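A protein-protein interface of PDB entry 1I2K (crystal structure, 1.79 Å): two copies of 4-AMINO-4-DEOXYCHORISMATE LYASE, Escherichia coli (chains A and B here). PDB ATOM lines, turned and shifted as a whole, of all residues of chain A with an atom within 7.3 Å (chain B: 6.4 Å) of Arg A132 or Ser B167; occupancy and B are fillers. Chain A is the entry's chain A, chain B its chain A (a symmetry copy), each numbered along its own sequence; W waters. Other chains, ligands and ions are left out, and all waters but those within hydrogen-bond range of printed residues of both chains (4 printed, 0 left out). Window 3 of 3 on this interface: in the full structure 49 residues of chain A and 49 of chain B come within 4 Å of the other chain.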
ATOM      1  N   ARG A 129     -23.585  -3.965 -18.286  1.00  0.00           N
ATOM      2  CA  ARG A 129     -23.568  -4.984 -17.248  1.00  0.00           C
ATOM      3  C   ARG A 129     -22.745  -4.575 -16.034  1.00  0.00           C
ATOM      4  O   ARG A 129     -21.610  -4.100 -16.155  1.00  0.00           O
ATOM      5  CB  ARG A 129     -22.995  -6.282 -17.845  1.00  0.00           C
ATOM      6  CG  ARG A 129     -24.027  -6.991 -18.716  1.00  0.00           C
ATOM      7  CD  ARG A 129     -23.372  -8.064 -19.570  1.00  0.00           C
ATOM      8  NE  ARG A 129     -24.374  -8.859 -20.277  1.00  0.00           N
ATOM      9  CZ  ARG A 129     -24.300 -10.180 -20.416  1.00  0.00           C
ATOM     10  NH1 ARG A 129     -23.284 -10.870 -19.914  1.00  0.00           N
ATOM     11  NH2 ARG A 129     -25.244 -10.845 -21.067  1.00  0.00           N
ATOM     12  N   LEU A 130     -23.305  -4.762 -14.840  1.00  0.00           N
ATOM     13  CA  LEU A 130     -22.642  -4.327 -13.616  1.00  0.00           C
ATOM     14  C   LEU A 130     -21.409  -5.138 -13.252  1.00  0.00           C
ATOM     15  O   LEU A 130     -21.437  -6.362 -13.302  1.00  0.00           O
ATOM     16  CB  LEU A 130     -23.578  -4.395 -12.402  1.00  0.00           C
ATOM     17  CG  LEU A 130     -24.926  -3.694 -12.521  1.00  0.00           C
ATOM     18  CD1 LEU A 130     -25.752  -4.011 -11.281  1.00  0.00           C
ATOM     19  CD2 LEU A 130     -24.738  -2.199 -12.739  1.00  0.00           C
ATOM     20  N   GLY A 131     -20.336  -4.427 -12.851  1.00  0.00           N
ATOM     21  CA  GLY A 131     -19.182  -5.151 -12.340  1.00  0.00           C
ATOM     22  C   GLY A 131     -19.555  -5.817 -11.016  1.00  0.00           C
ATOM     23  O   GLY A 131     -20.450  -5.373 -10.288  1.00  0.00           O
ATOM     24  N   ARG A 132     -18.865  -6.901 -10.701  1.00  0.00           N
ATOM     25  CA  ARG A 132     -19.092  -7.634  -9.451  1.00  0.00           C
ATOM     26  C   ARG A 132     -17.999  -7.289  -8.444  1.00  0.00           C
ATOM     27  O   ARG A 132     -16.822  -7.452  -8.770  1.00  0.00           O
ATOM     28  CB  ARG A 132     -19.084  -9.146  -9.746  1.00  0.00           C
ATOM     29  CG  ARG A 132     -20.316  -9.562 -10.539  1.00  0.00           C
ATOM     30  CD  ARG A 132     -20.140 -10.887 -11.248  1.00  0.00           C
ATOM     31  NE  ARG A 132     -19.721 -11.975 -10.359  1.00  0.00           N
ATOM     32  CZ  ARG A 132     -20.550 -12.754  -9.676  1.00  0.00           C
ATOM     33  NH1 ARG A 132     -21.864 -12.563  -9.770  1.00  0.00           N
ATOM     34  NH2 ARG A 132     -20.093 -13.730  -8.889  1.00  0.00           N
ATOM     35  N   ASN A 133     -18.347  -6.806  -7.262  1.00  0.00           N
ATOM     36  CA  ASN A 133     -17.390  -6.465  -6.216  1.00  0.00           C
ATOM     37  C   ASN A 133     -18.063  -6.535  -4.857  1.00  0.00           C
ATOM     38  O   ASN A 133     -18.809  -5.645  -4.440  1.00  0.00           O
ATOM     39  CB  ASN A 133     -16.811  -5.053  -6.397  1.00  0.00           C
ATOM     40  CG  ASN A 133     -15.677  -4.782  -5.431  1.00  0.00           C
ATOM     41  OD1 ASN A 133     -15.505  -5.482  -4.436  1.00  0.00           O
ATOM     42  ND2 ASN A 133     -14.872  -3.771  -5.760  1.00  0.00           N
ATOM     43  N   PRO A 134     -17.832  -7.622  -4.131  1.00  0.00           N
ATOM     44  CA  PRO A 134     -18.573  -7.795  -2.886  1.00  0.00           C
ATOM     45  C   PRO A 134     -18.216  -6.730  -1.848  1.00  0.00           C
ATOM     46  O   PRO A 134     -18.934  -6.548  -0.854  1.00  0.00           O
ATOM     47  CB  PRO A 134     -18.128  -9.182  -2.390  1.00  0.00           C
ATOM     48  CG  PRO A 134     -16.961  -9.582  -3.222  1.00  0.00           C
ATOM     49  CD  PRO A 134     -16.910  -8.722  -4.457  1.00  0.00           C
ATOM     50  N   HIS A 135     -17.102  -6.028  -2.047  1.00  0.00           N
ATOM     51  CA  HIS A 135     -16.721  -5.002  -1.091  1.00  0.00           C
ATOM     52  C   HIS A 135     -17.628  -3.793  -1.166  1.00  0.00           C
ATOM     53  O   HIS A 135     -17.749  -3.030  -0.196  1.00  0.00           O
ATOM     54  CB  HIS A 135     -15.272  -4.542  -1.339  1.00  0.00           C
ATOM     55  CG  HIS A 135     -14.274  -5.450  -0.693  1.00  0.00           C
ATOM     56  ND1 HIS A 135     -13.881  -5.335   0.629  1.00  0.00           N
ATOM     57  CD2 HIS A 135     -13.593  -6.502  -1.210  1.00  0.00           C
ATOM     58  CE1 HIS A 135     -12.991  -6.279   0.890  1.00  0.00           C
ATOM     59  NE2 HIS A 135     -12.802  -7.000  -0.201  1.00  0.00           N
ATOM     60  N   LEU A 136     -18.227  -3.624  -2.351  1.00  0.00           N
ATOM     61  CA  LEU A 136     -19.181  -2.505  -2.453  1.00  0.00           C
ATOM     62  C   LEU A 136     -20.615  -2.964  -2.633  1.00  0.00           C
ATOM     63  O   LEU A 136     -21.541  -2.146  -2.610  1.00  0.00           O
ATOM     64  CB  LEU A 136     -18.790  -1.618  -3.642  1.00  0.00           C
ATOM     65  CG  LEU A 136     -17.543  -0.764  -3.507  1.00  0.00           C
ATOM     66  CD1 LEU A 136     -17.230  -0.129  -4.866  1.00  0.00           C
ATOM     67  CD2 LEU A 136     -17.683   0.301  -2.421  1.00  0.00           C
ATOM     68  N   ALA A 137     -20.845  -4.278  -2.804  1.00  0.00           N
ATOM     69  CA  ALA A 137     -22.200  -4.710  -3.152  1.00  0.00           C
ATOM     70  C   ALA A 137     -23.237  -4.408  -2.083  1.00  0.00           C
ATOM     71  O   ALA A 137     -22.988  -4.584  -0.880  1.00  0.00           O
ATOM     72  CB  ALA A 137     -22.193  -6.222  -3.435  1.00  0.00           C
ATOM     73  N   GLU A 146     -22.348   3.731 -13.265  1.00  0.00           N
ATOM     74  CA  GLU A 146     -22.942   2.599 -14.001  1.00  0.00           C
ATOM     75  C   GLU A 146     -24.424   2.876 -14.262  1.00  0.00           C
ATOM     76  O   GLU A 146     -24.924   2.610 -15.348  1.00  0.00           O
ATOM     77  CB  GLU A 146     -22.748   1.281 -13.250  1.00  0.00           C
ATOM     78  CG  GLU A 146     -21.314   0.763 -13.296  1.00  0.00           C
ATOM     79  CD  GLU A 146     -21.107  -0.577 -12.624  1.00  0.00           C
ATOM     80  OE1 GLU A 146     -21.599  -0.828 -11.506  1.00  0.00           O
ATOM     81  OE2 GLU A 146     -20.389  -1.427 -13.222  1.00  0.00           O
ATOM     82  N   ASP A 166     -25.346  -8.713 -14.246  1.00  0.00           N
ATOM     83  CA  ASP A 166     -23.952  -8.396 -13.887  1.00  0.00           C
ATOM     84  C   ASP A 166     -22.965  -8.960 -14.920  1.00  0.00           C
ATOM     85  O   ASP A 166     -23.416  -9.468 -15.957  1.00  0.00           O
ATOM     86  CB  ASP A 166     -23.604  -8.879 -12.488  1.00  0.00           C
ATOM     87  CG  ASP A 166     -23.548 -10.371 -12.280  1.00  0.00           C
ATOM     88  OD1 ASP A 166     -23.427 -11.135 -13.254  1.00  0.00           O
ATOM     89  OD2 ASP A 166     -23.649 -10.815 -11.107  1.00  0.00           O
ATOM     90  N   SER A 167     -21.663  -8.868 -14.664  1.00  0.00           N
ATOM     91  CA  SER A 167     -20.675  -9.253 -15.672  1.00  0.00           C
ATOM     92  C   SER A 167     -20.704 -10.769 -15.953  1.00  0.00           C
ATOM     93  O   SER A 167     -20.140 -11.215 -16.969  1.00  0.00           O
ATOM     94  CB  SER A 167     -19.248  -8.894 -15.280  1.00  0.00           C
ATOM     95  OG  SER A 167     -18.835  -9.584 -14.101  1.00  0.00           O
ATOM     96  N   GLU A 168     -21.340 -11.535 -15.079  1.00  0.00           N
ATOM     97  CA  GLU A 168     -21.452 -12.974 -15.305  1.00  0.00           C
ATOM     98  C   GLU A 168     -22.753 -13.355 -16.003  1.00  0.00           C
ATOM     99  O   GLU A 168     -23.032 -14.530 -16.283  1.00  0.00           O
ATOM    100  CB  GLU A 168     -21.375 -13.740 -13.977  1.00  0.00           C
ATOM    101  CG  GLU A 168     -19.979 -13.690 -13.349  1.00  0.00           C
ATOM    102  CD  GLU A 168     -19.077 -14.748 -13.956  1.00  0.00           C
ATOM    103  OE1 GLU A 168     -19.071 -15.884 -13.447  1.00  0.00           O
ATOM    104  OE2 GLU A 168     -18.384 -14.442 -14.941  1.00  0.00           O
ATOM    105  N   GLY A 169     -23.574 -12.360 -16.292  1.00  0.00           N
ATOM    106  CA  GLY A 169     -24.867 -12.560 -16.911  1.00  0.00           C
ATOM    107  C   GLY A 169     -26.016 -12.788 -15.953  1.00  0.00           C
ATOM    108  O   GLY A 169     -27.122 -13.068 -16.456  1.00  0.00           O
ATOM    109  N   TRP A 170     -25.838 -12.673 -14.639  1.00  0.00           N
ATOM    110  CA  TRP A 170     -26.952 -12.870 -13.718  1.00  0.00           C
ATOM    111  C   TRP A 170     -27.820 -11.623 -13.517  1.00  0.00           C
ATOM    112  O   TRP A 170     -27.287 -10.542 -13.259  1.00  0.00           O
ATOM    113  CB  TRP A 170     -26.499 -13.295 -12.319  1.00  0.00           C
ATOM    114  CG  TRP A 170     -25.514 -14.423 -12.280  1.00  0.00           C
ATOM    115  CD1 TRP A 170     -24.224 -14.361 -11.841  1.00  0.00           C
ATOM    116  CD2 TRP A 170     -25.742 -15.777 -12.701  1.00  0.00           C
ATOM    117  NE1 TRP A 170     -23.633 -15.608 -11.964  1.00  0.00           N
ATOM    118  CE2 TRP A 170     -24.544 -16.486 -12.487  1.00  0.00           C
ATOM    119  CE3 TRP A 170     -26.844 -16.450 -13.237  1.00  0.00           C
ATOM    120  CZ2 TRP A 170     -24.427 -17.843 -12.793  1.00  0.00           C
ATOM    121  CZ3 TRP A 170     -26.724 -17.801 -13.540  1.00  0.00           C
ATOM    122  CH2 TRP A 170     -25.521 -18.481 -13.316  1.00  0.00           C
ATOM    123  N   THR A 172     -29.704  -8.886 -11.885  1.00  0.00           N
ATOM    124  CA  THR A 172     -29.368  -8.274 -10.594  1.00  0.00           C
ATOM    125  C   THR A 172     -30.427  -7.277 -10.155  1.00  0.00           C
ATOM    126  O   THR A 172     -30.927  -7.407  -9.031  1.00  0.00           O
ATOM    127  CB  THR A 172     -28.002  -7.563 -10.704  1.00  0.00           C
ATOM    128  OG1 THR A 172     -27.023  -8.539 -11.072  1.00  0.00           O
ATOM    129  CG2 THR A 172     -27.580  -6.946  -9.379  1.00  0.00           C
ATOM    130  N   ARG A 191     -30.020 -12.230  -5.460  1.00  0.00           N
ATOM    131  CA  ARG A 191     -29.120 -12.056  -4.323  1.00  0.00           C
ATOM    132  C   ARG A 191     -28.185 -10.907  -4.669  1.00  0.00           C
ATOM    133  O   ARG A 191     -27.698 -10.884  -5.797  1.00  0.00           O
ATOM    134  CB  ARG A 191     -28.339 -13.313  -3.972  1.00  0.00           C
ATOM    135  CG  ARG A 191     -28.294 -14.426  -5.000  1.00  0.00           C
ATOM    136  CD  ARG A 191     -27.825 -15.743  -4.377  1.00  0.00           C
ATOM    137  NE  ARG A 191     -26.470 -15.648  -3.837  1.00  0.00           N
ATOM    138  CZ  ARG A 191     -25.380 -16.196  -4.348  1.00  0.00           C
ATOM    139  NH1 ARG A 191     -25.411 -16.925  -5.455  1.00  0.00           N
ATOM    140  NH2 ARG A 191     -24.208 -16.023  -3.741  1.00  0.00           N
ATOM    141  N   ASP A 193     -25.182  -9.925  -3.169  1.00  0.00           N
ATOM    142  CA  ASP A 193     -23.887  -9.982  -2.497  1.00  0.00           C
ATOM    143  C   ASP A 193     -22.696  -9.639  -3.395  1.00  0.00           C
ATOM    144  O   ASP A 193     -21.571  -9.437  -2.906  1.00  0.00           O
ATOM    145  CB  ASP A 193     -23.736 -11.404  -1.937  1.00  0.00           C
ATOM    146  CG  ASP A 193     -23.726 -12.453  -3.032  1.00  0.00           C
ATOM    147  OD1 ASP A 193     -24.527 -12.393  -4.005  1.00  0.00           O
ATOM    148  OD2 ASP A 193     -22.885 -13.376  -2.905  1.00  0.00           O
ATOM    149  N   GLN A 194     -22.893  -9.569  -4.705  1.00  0.00           N
ATOM    150  CA  GLN A 194     -21.821  -9.323  -5.682  1.00  0.00           C
ATOM    151  C   GLN A 194     -22.052  -7.993  -6.407  1.00  0.00           C
ATOM    152  O   GLN A 194     -21.100  -7.305  -6.790  1.00  0.00           O
ATOM    153  CB  GLN A 194     -21.717 -10.455  -6.701  1.00  0.00           C
ATOM    154  CG  GLN A 194     -21.245 -11.749  -6.051  1.00  0.00           C
ATOM    155  CD  GLN A 194     -19.806 -11.687  -5.586  1.00  0.00           C
ATOM    156  OE1 GLN A 194     -19.439 -12.305  -4.589  1.00  0.00           O
ATOM    157  NE2 GLN A 194     -18.949 -10.954  -6.283  1.00  0.00           N
ATOM    158  N   ALA A 195     -23.313  -7.604  -6.591  1.00  0.00           N
ATOM    159  CA  ALA A 195     -23.612  -6.307  -7.196  1.00  0.00           C
ATOM    160  C   ALA A 195     -25.012  -5.829  -6.835  1.00  0.00           C
ATOM    161  O   ALA A 195     -25.848  -6.592  -6.344  1.00  0.00           O
ATOM    162  CB  ALA A 195     -23.468  -6.387  -8.707  1.00  0.00           C
ATOM    163  N   GLN A 220     -29.536 -16.593  -7.861  1.00  0.00           N
ATOM    164  CA  GLN A 220     -28.689 -16.261  -8.995  1.00  0.00           C
ATOM    165  C   GLN A 220     -29.332 -16.820 -10.261  1.00  0.00           C
ATOM    166  O   GLN A 220     -29.284 -18.037 -10.453  1.00  0.00           O
ATOM    167  CB  GLN A 220     -27.295 -16.857  -8.829  1.00  0.00           C
ATOM    168  CG  GLN A 220     -26.263 -15.925  -8.208  1.00  0.00           C
ATOM    169  CD  GLN A 220     -24.867 -16.500  -8.386  1.00  0.00           C
ATOM    170  OE1 GLN A 220     -23.961 -15.792  -8.815  1.00  0.00           O
ATOM    171  NE2 GLN A 220     -24.731 -17.782  -8.057  1.00  0.00           N
ATOM    172  N   ARG B 129     -10.847  -6.677  -5.152  1.00  0.00           N
ATOM    173  CA  ARG B 129     -10.757  -6.992  -6.569  1.00  0.00           C
ATOM    174  C   ARG B 129     -11.681  -6.135  -7.424  1.00  0.00           C
ATOM    175  O   ARG B 129     -12.868  -5.967  -7.120  1.00  0.00           O
ATOM    176  CB  ARG B 129     -11.107  -8.478  -6.764  1.00  0.00           C
ATOM    177  CG  ARG B 129      -9.946  -9.376  -6.350  1.00  0.00           C
ATOM    178  CD  ARG B 129     -10.398 -10.821  -6.212  1.00  0.00           C
ATOM    179  NE  ARG B 129      -9.262 -11.710  -5.984  1.00  0.00           N
ATOM    180  CZ  ARG B 129      -9.133 -12.902  -6.559  1.00  0.00           C
ATOM    181  NH1 ARG B 129     -10.056 -13.369  -7.390  1.00  0.00           N
ATOM    182  NH2 ARG B 129      -8.075 -13.662  -6.313  1.00  0.00           N
ATOM    183  N   LEU B 130     -11.151  -5.585  -8.514  1.00  0.00           N
ATOM    184  CA  LEU B 130     -11.921  -4.677  -9.357  1.00  0.00           C
ATOM    185  C   LEU B 130     -13.035  -5.350 -10.143  1.00  0.00           C
ATOM    186  O   LEU B 130     -12.825  -6.399 -10.738  1.00  0.00           O
ATOM    187  CB  LEU B 130     -11.038  -3.961 -10.386  1.00  0.00           C
ATOM    188  CG  LEU B 130      -9.805  -3.236  -9.862  1.00  0.00           C
ATOM    189  CD1 LEU B 130      -8.993  -2.732 -11.048  1.00  0.00           C
ATOM    190  CD2 LEU B 130     -10.202  -2.123  -8.902  1.00  0.00           C
ATOM    191  N   GLY B 131     -14.218  -4.702 -10.156  1.00  0.00           N
ATOM    192  CA  GLY B 131     -15.272  -5.213 -11.019  1.00  0.00           C
ATOM    193  C   GLY B 131     -14.861  -5.024 -12.479  1.00  0.00           C
ATOM    194  O   GLY B 131     -14.073  -4.139 -12.829  1.00  0.00           O
ATOM    195  N   ARG B 132     -15.396  -5.871 -13.343  1.00  0.00           N
ATOM    196  CA  ARG B 132     -15.116  -5.800 -14.781  1.00  0.00           C
ATOM    197  C   ARG B 132     -16.290  -5.144 -15.503  1.00  0.00           C
ATOM    198  O   ARG B 132     -17.415  -5.625 -15.361  1.00  0.00           O
ATOM    199  CB  ARG B 132     -14.888  -7.224 -15.321  1.00  0.00           C
ATOM    200  CG  ARG B 132     -13.576  -7.806 -14.812  1.00  0.00           C
ATOM    201  CD  ARG B 132     -13.525  -9.315 -14.909  1.00  0.00           C
ATOM    202  NE  ARG B 132     -13.816  -9.825 -16.252  1.00  0.00           N
ATOM    203  CZ  ARG B 132     -12.910 -10.000 -17.207  1.00  0.00           C
ATOM    204  NH1 ARG B 132     -11.636  -9.694 -16.971  1.00  0.00           N
ATOM    205  NH2 ARG B 132     -13.251 -10.474 -18.405  1.00  0.00           N
ATOM    206  N   GLU B 146     -13.417   2.226  -5.453  1.00  0.00           N
ATOM    207  CA  GLU B 146     -12.632   0.979  -5.394  1.00  0.00           C
ATOM    208  C   GLU B 146     -11.197   1.294  -4.965  1.00  0.00           C
ATOM    209  O   GLU B 146     -10.618   0.577  -4.158  1.00  0.00           O
ATOM    210  CB  GLU B 146     -12.660   0.237  -6.730  1.00  0.00           C
ATOM    211  CG  GLU B 146     -13.999  -0.434  -7.022  1.00  0.00           C
ATOM    212  CD  GLU B 146     -14.034  -1.238  -8.304  1.00  0.00           C
ATOM    213  OE1 GLU B 146     -13.558  -0.791  -9.367  1.00  0.00           O
ATOM    214  OE2 GLU B 146     -14.593  -2.369  -8.270  1.00  0.00           O
ATOM    215  N   LEU B 165      -5.933  -7.199  -8.676  1.00  0.00           N
ATOM    216  CA  LEU B 165      -6.561  -8.115  -9.608  1.00  0.00           C
ATOM    217  C   LEU B 165      -8.007  -7.764  -9.910  1.00  0.00           C
ATOM    218  O   LEU B 165      -8.648  -7.039  -9.131  1.00  0.00           O
ATOM    219  CB  LEU B 165      -6.567  -9.533  -9.030  1.00  0.00           C
ATOM    220  CG  LEU B 165      -5.297  -9.982  -8.310  1.00  0.00           C
ATOM    221  CD1 LEU B 165      -5.550 -11.284  -7.566  1.00  0.00           C
ATOM    222  CD2 LEU B 165      -4.161 -10.136  -9.300  1.00  0.00           C
ATOM    223  N   ASP B 166      -8.575  -8.289 -11.001  1.00  0.00           N
ATOM    224  CA  ASP B 166     -10.015  -8.042 -11.199  1.00  0.00           C
ATOM    225  C   ASP B 166     -10.864  -9.201 -10.656  1.00  0.00           C
ATOM    226  O   ASP B 166     -10.300 -10.104 -10.020  1.00  0.00           O
ATOM    227  CB  ASP B 166     -10.347  -7.766 -12.657  1.00  0.00           C
ATOM    228  CG  ASP B 166     -10.189  -8.919 -13.617  1.00  0.00           C
ATOM    229  OD1 ASP B 166     -10.156 -10.087 -13.193  1.00  0.00           O
ATOM    230  OD2 ASP B 166     -10.074  -8.663 -14.844  1.00  0.00           O
ATOM    231  N   SER B 167     -12.174  -9.183 -10.880  1.00  0.00           N
ATOM    232  CA  SER B 167     -13.052 -10.179 -10.265  1.00  0.00           C
ATOM    233  C   SER B 167     -12.787 -11.594 -10.817  1.00  0.00           C
ATOM    234  O   SER B 167     -13.236 -12.583 -10.210  1.00  0.00           O
ATOM    235  CB  SER B 167     -14.532  -9.883 -10.471  1.00  0.00           C
ATOM    236  OG  SER B 167     -14.887  -9.906 -11.853  1.00  0.00           O
ATOM    237  N   GLU B 168     -12.083 -11.685 -11.936  1.00  0.00           N
ATOM    238  CA  GLU B 168     -11.750 -12.995 -12.491  1.00  0.00           C
ATOM    239  C   GLU B 168     -10.379 -13.488 -12.042  1.00  0.00           C
ATOM    240  O   GLU B 168      -9.917 -14.579 -12.406  1.00  0.00           O
ATOM    241  CB  GLU B 168     -11.768 -12.955 -14.026  1.00  0.00           C
ATOM    242  CG  GLU B 168     -13.182 -12.791 -14.593  1.00  0.00           C
ATOM    243  CD  GLU B 168     -13.891 -14.130 -14.667  1.00  0.00           C
ATOM    244  OE1 GLU B 168     -13.751 -14.818 -15.695  1.00  0.00           O
ATOM    245  OE2 GLU B 168     -14.580 -14.490 -13.698  1.00  0.00           O
ATOM    246  N   GLY B 169      -9.702 -12.682 -11.241  1.00  0.00           N
ATOM    247  CA  GLY B 169      -8.369 -12.983 -10.765  1.00  0.00           C
ATOM    248  C   GLY B 169      -7.240 -12.504 -11.650  1.00  0.00           C
ATOM    249  O   GLY B 169      -6.084 -12.839 -11.323  1.00  0.00           O
ATOM    250  N   TRP B 170      -7.488 -11.746 -12.717  1.00  0.00           N
ATOM    251  CA  TRP B 170      -6.397 -11.265 -13.557  1.00  0.00           C
ATOM    252  C   TRP B 170      -5.731  -9.986 -13.040  1.00  0.00           C
ATOM    253  O   TRP B 170      -6.429  -9.022 -12.716  1.00  0.00           O
ATOM    254  CB  TRP B 170      -6.841 -10.957 -14.989  1.00  0.00           C
ATOM    255  CG  TRP B 170      -7.649 -12.029 -15.654  1.00  0.00           C
ATOM    256  CD1 TRP B 170      -8.951 -11.938 -16.049  1.00  0.00           C
ATOM    257  CD2 TRP B 170      -7.206 -13.353 -15.994  1.00  0.00           C
ATOM    258  NE1 TRP B 170      -9.346 -13.136 -16.622  1.00  0.00           N
ATOM    259  CE2 TRP B 170      -8.294 -14.013 -16.597  1.00  0.00           C
ATOM    260  CE3 TRP B 170      -5.995 -14.035 -15.844  1.00  0.00           C
ATOM    261  CZ2 TRP B 170      -8.197 -15.329 -17.052  1.00  0.00           C
ATOM    262  CZ3 TRP B 170      -5.902 -15.345 -16.297  1.00  0.00           C
ATOM    263  CH2 TRP B 170      -6.999 -15.977 -16.894  1.00  0.00           C
HETATM  264  O   HOH W   1     -14.407  -7.959  -7.425  1.00  0.00           O
HETATM  265  O   HOH W   2     -13.394  -7.286  -4.023  1.00  0.00           O
HETATM  266  O   HOH W   3     -19.783  -5.704 -16.872  1.00  0.00           O
HETATM  267  O   HOH W   4     -16.980  -8.265 -12.557  1.00  0.00           O
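ND2 of Asn A133 is in hydrogen-bond range of O of Arg B129 (3.3 Å). ND2 of Asn A133 sits at hydrogen-bond distance from OE2 of Glu B146, at 2.9 Å.
O of Leu A130 sits at hydrogen-bond distance from N of Ser A167, 2.9 Å away. OD2 of Asp A166 lies within salt-bridge range of NH1 of Arg A132 (2.8 Å). OD1 of Asn A133 is in hydrogen-bond range of N of His A135 (2.9 Å). The backbone carbonyl oxygen (O) of Leu B130 sits at hydrogen-bond distance from the backbone NH (N) of Ser B167, 2.9 Å away. The backbone NH (N) of Gly B131 is in hydrogen-bond range of the side-chain carboxylate (OE2) of Glu B146, 3.0 Å away. The guanidinium group (NH1) of Arg B132 is in salt-bridge range of the side-chain carboxylate (OD2) of Asp B166, 2.8 Å away.
Among the printed residues, pairs that only touch across the chains: Gly A131 with Arg B132, Arg A132 with Gly B131, Arg A132 with Ser B167, Leu A136 with Glu B146 and Ser A167 with Arg B132.
Arg A132 touches just these residues of chain B: Gly B131 and Ser B167. Of the printed residues of chain B, Leu A136 touches Glu B146 (3.9 Å). Asp A193 touches none of the printed residues of chain B. Of the printed residues of chain A, Arg B129 touches Asn A133 (3.3 Å). Printed residues of chain A within 4 Å of Arg B132: Gly A131 (3.5 Å) and Ser A167 (3.7 Å). The nearest printed residue of chain B that does not touch Ser A167 is Ser B167 (4.6 Å).
Printed residues of chain B that touch a printed residue of chain A: Arg B129, Gly B131, Arg B132, Glu B146 and Ser B167. Hydrophobic or aromatic side chains of chain A within 4 Å of the printed part of chain B: Leu A136. Among the printed residues, 7 pairs touch across the chains. Among the printed residues, no Asp or Glu carboxylate lies within 4 Å of a Lys or Arg side-chain nitrogen of the other chain.
Gly A131 touches Arg B132, and with the chains exchanged Arg A132 touches Gly B131. Arg A132 touches Ser B167, and with the chains exchanged Ser A167 touches Arg B132. 10 positions are printed for both chains. Of the 7 pairs that touch across the chains among the printed residues, 4 have their exchanged pair printed and touching as well.
Water W3 lies within hydrogen-bond range of the backbone carbonyl oxygen of Arg A129 (2.5 Å) and the backbone carbonyl oxygen of Arg B132 (2.8 Å). Water W1 lies within hydrogen-bond range of the backbone carbonyl oxygen (O) of Arg B129 (2.5 Å) and the backbone carbonyl oxygen (O) of Arg A132 (2.8 Å). Water W4 lies within hydrogen-bond range of the side-chain hydroxyl (OG) of Ser A167 (2.8 Å), the side-chain hydroxyl (OG) of Ser B167 (2.8 Å), the backbone NH (N) of Arg B132 (3.0 Å) and the backbone NH (N) of Arg A132 (3.0 Å). Water W2 lies within hydrogen-bond range of OD1 of Asn A133 (2.8 Å) and N of Arg B129 (2.9 Å).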
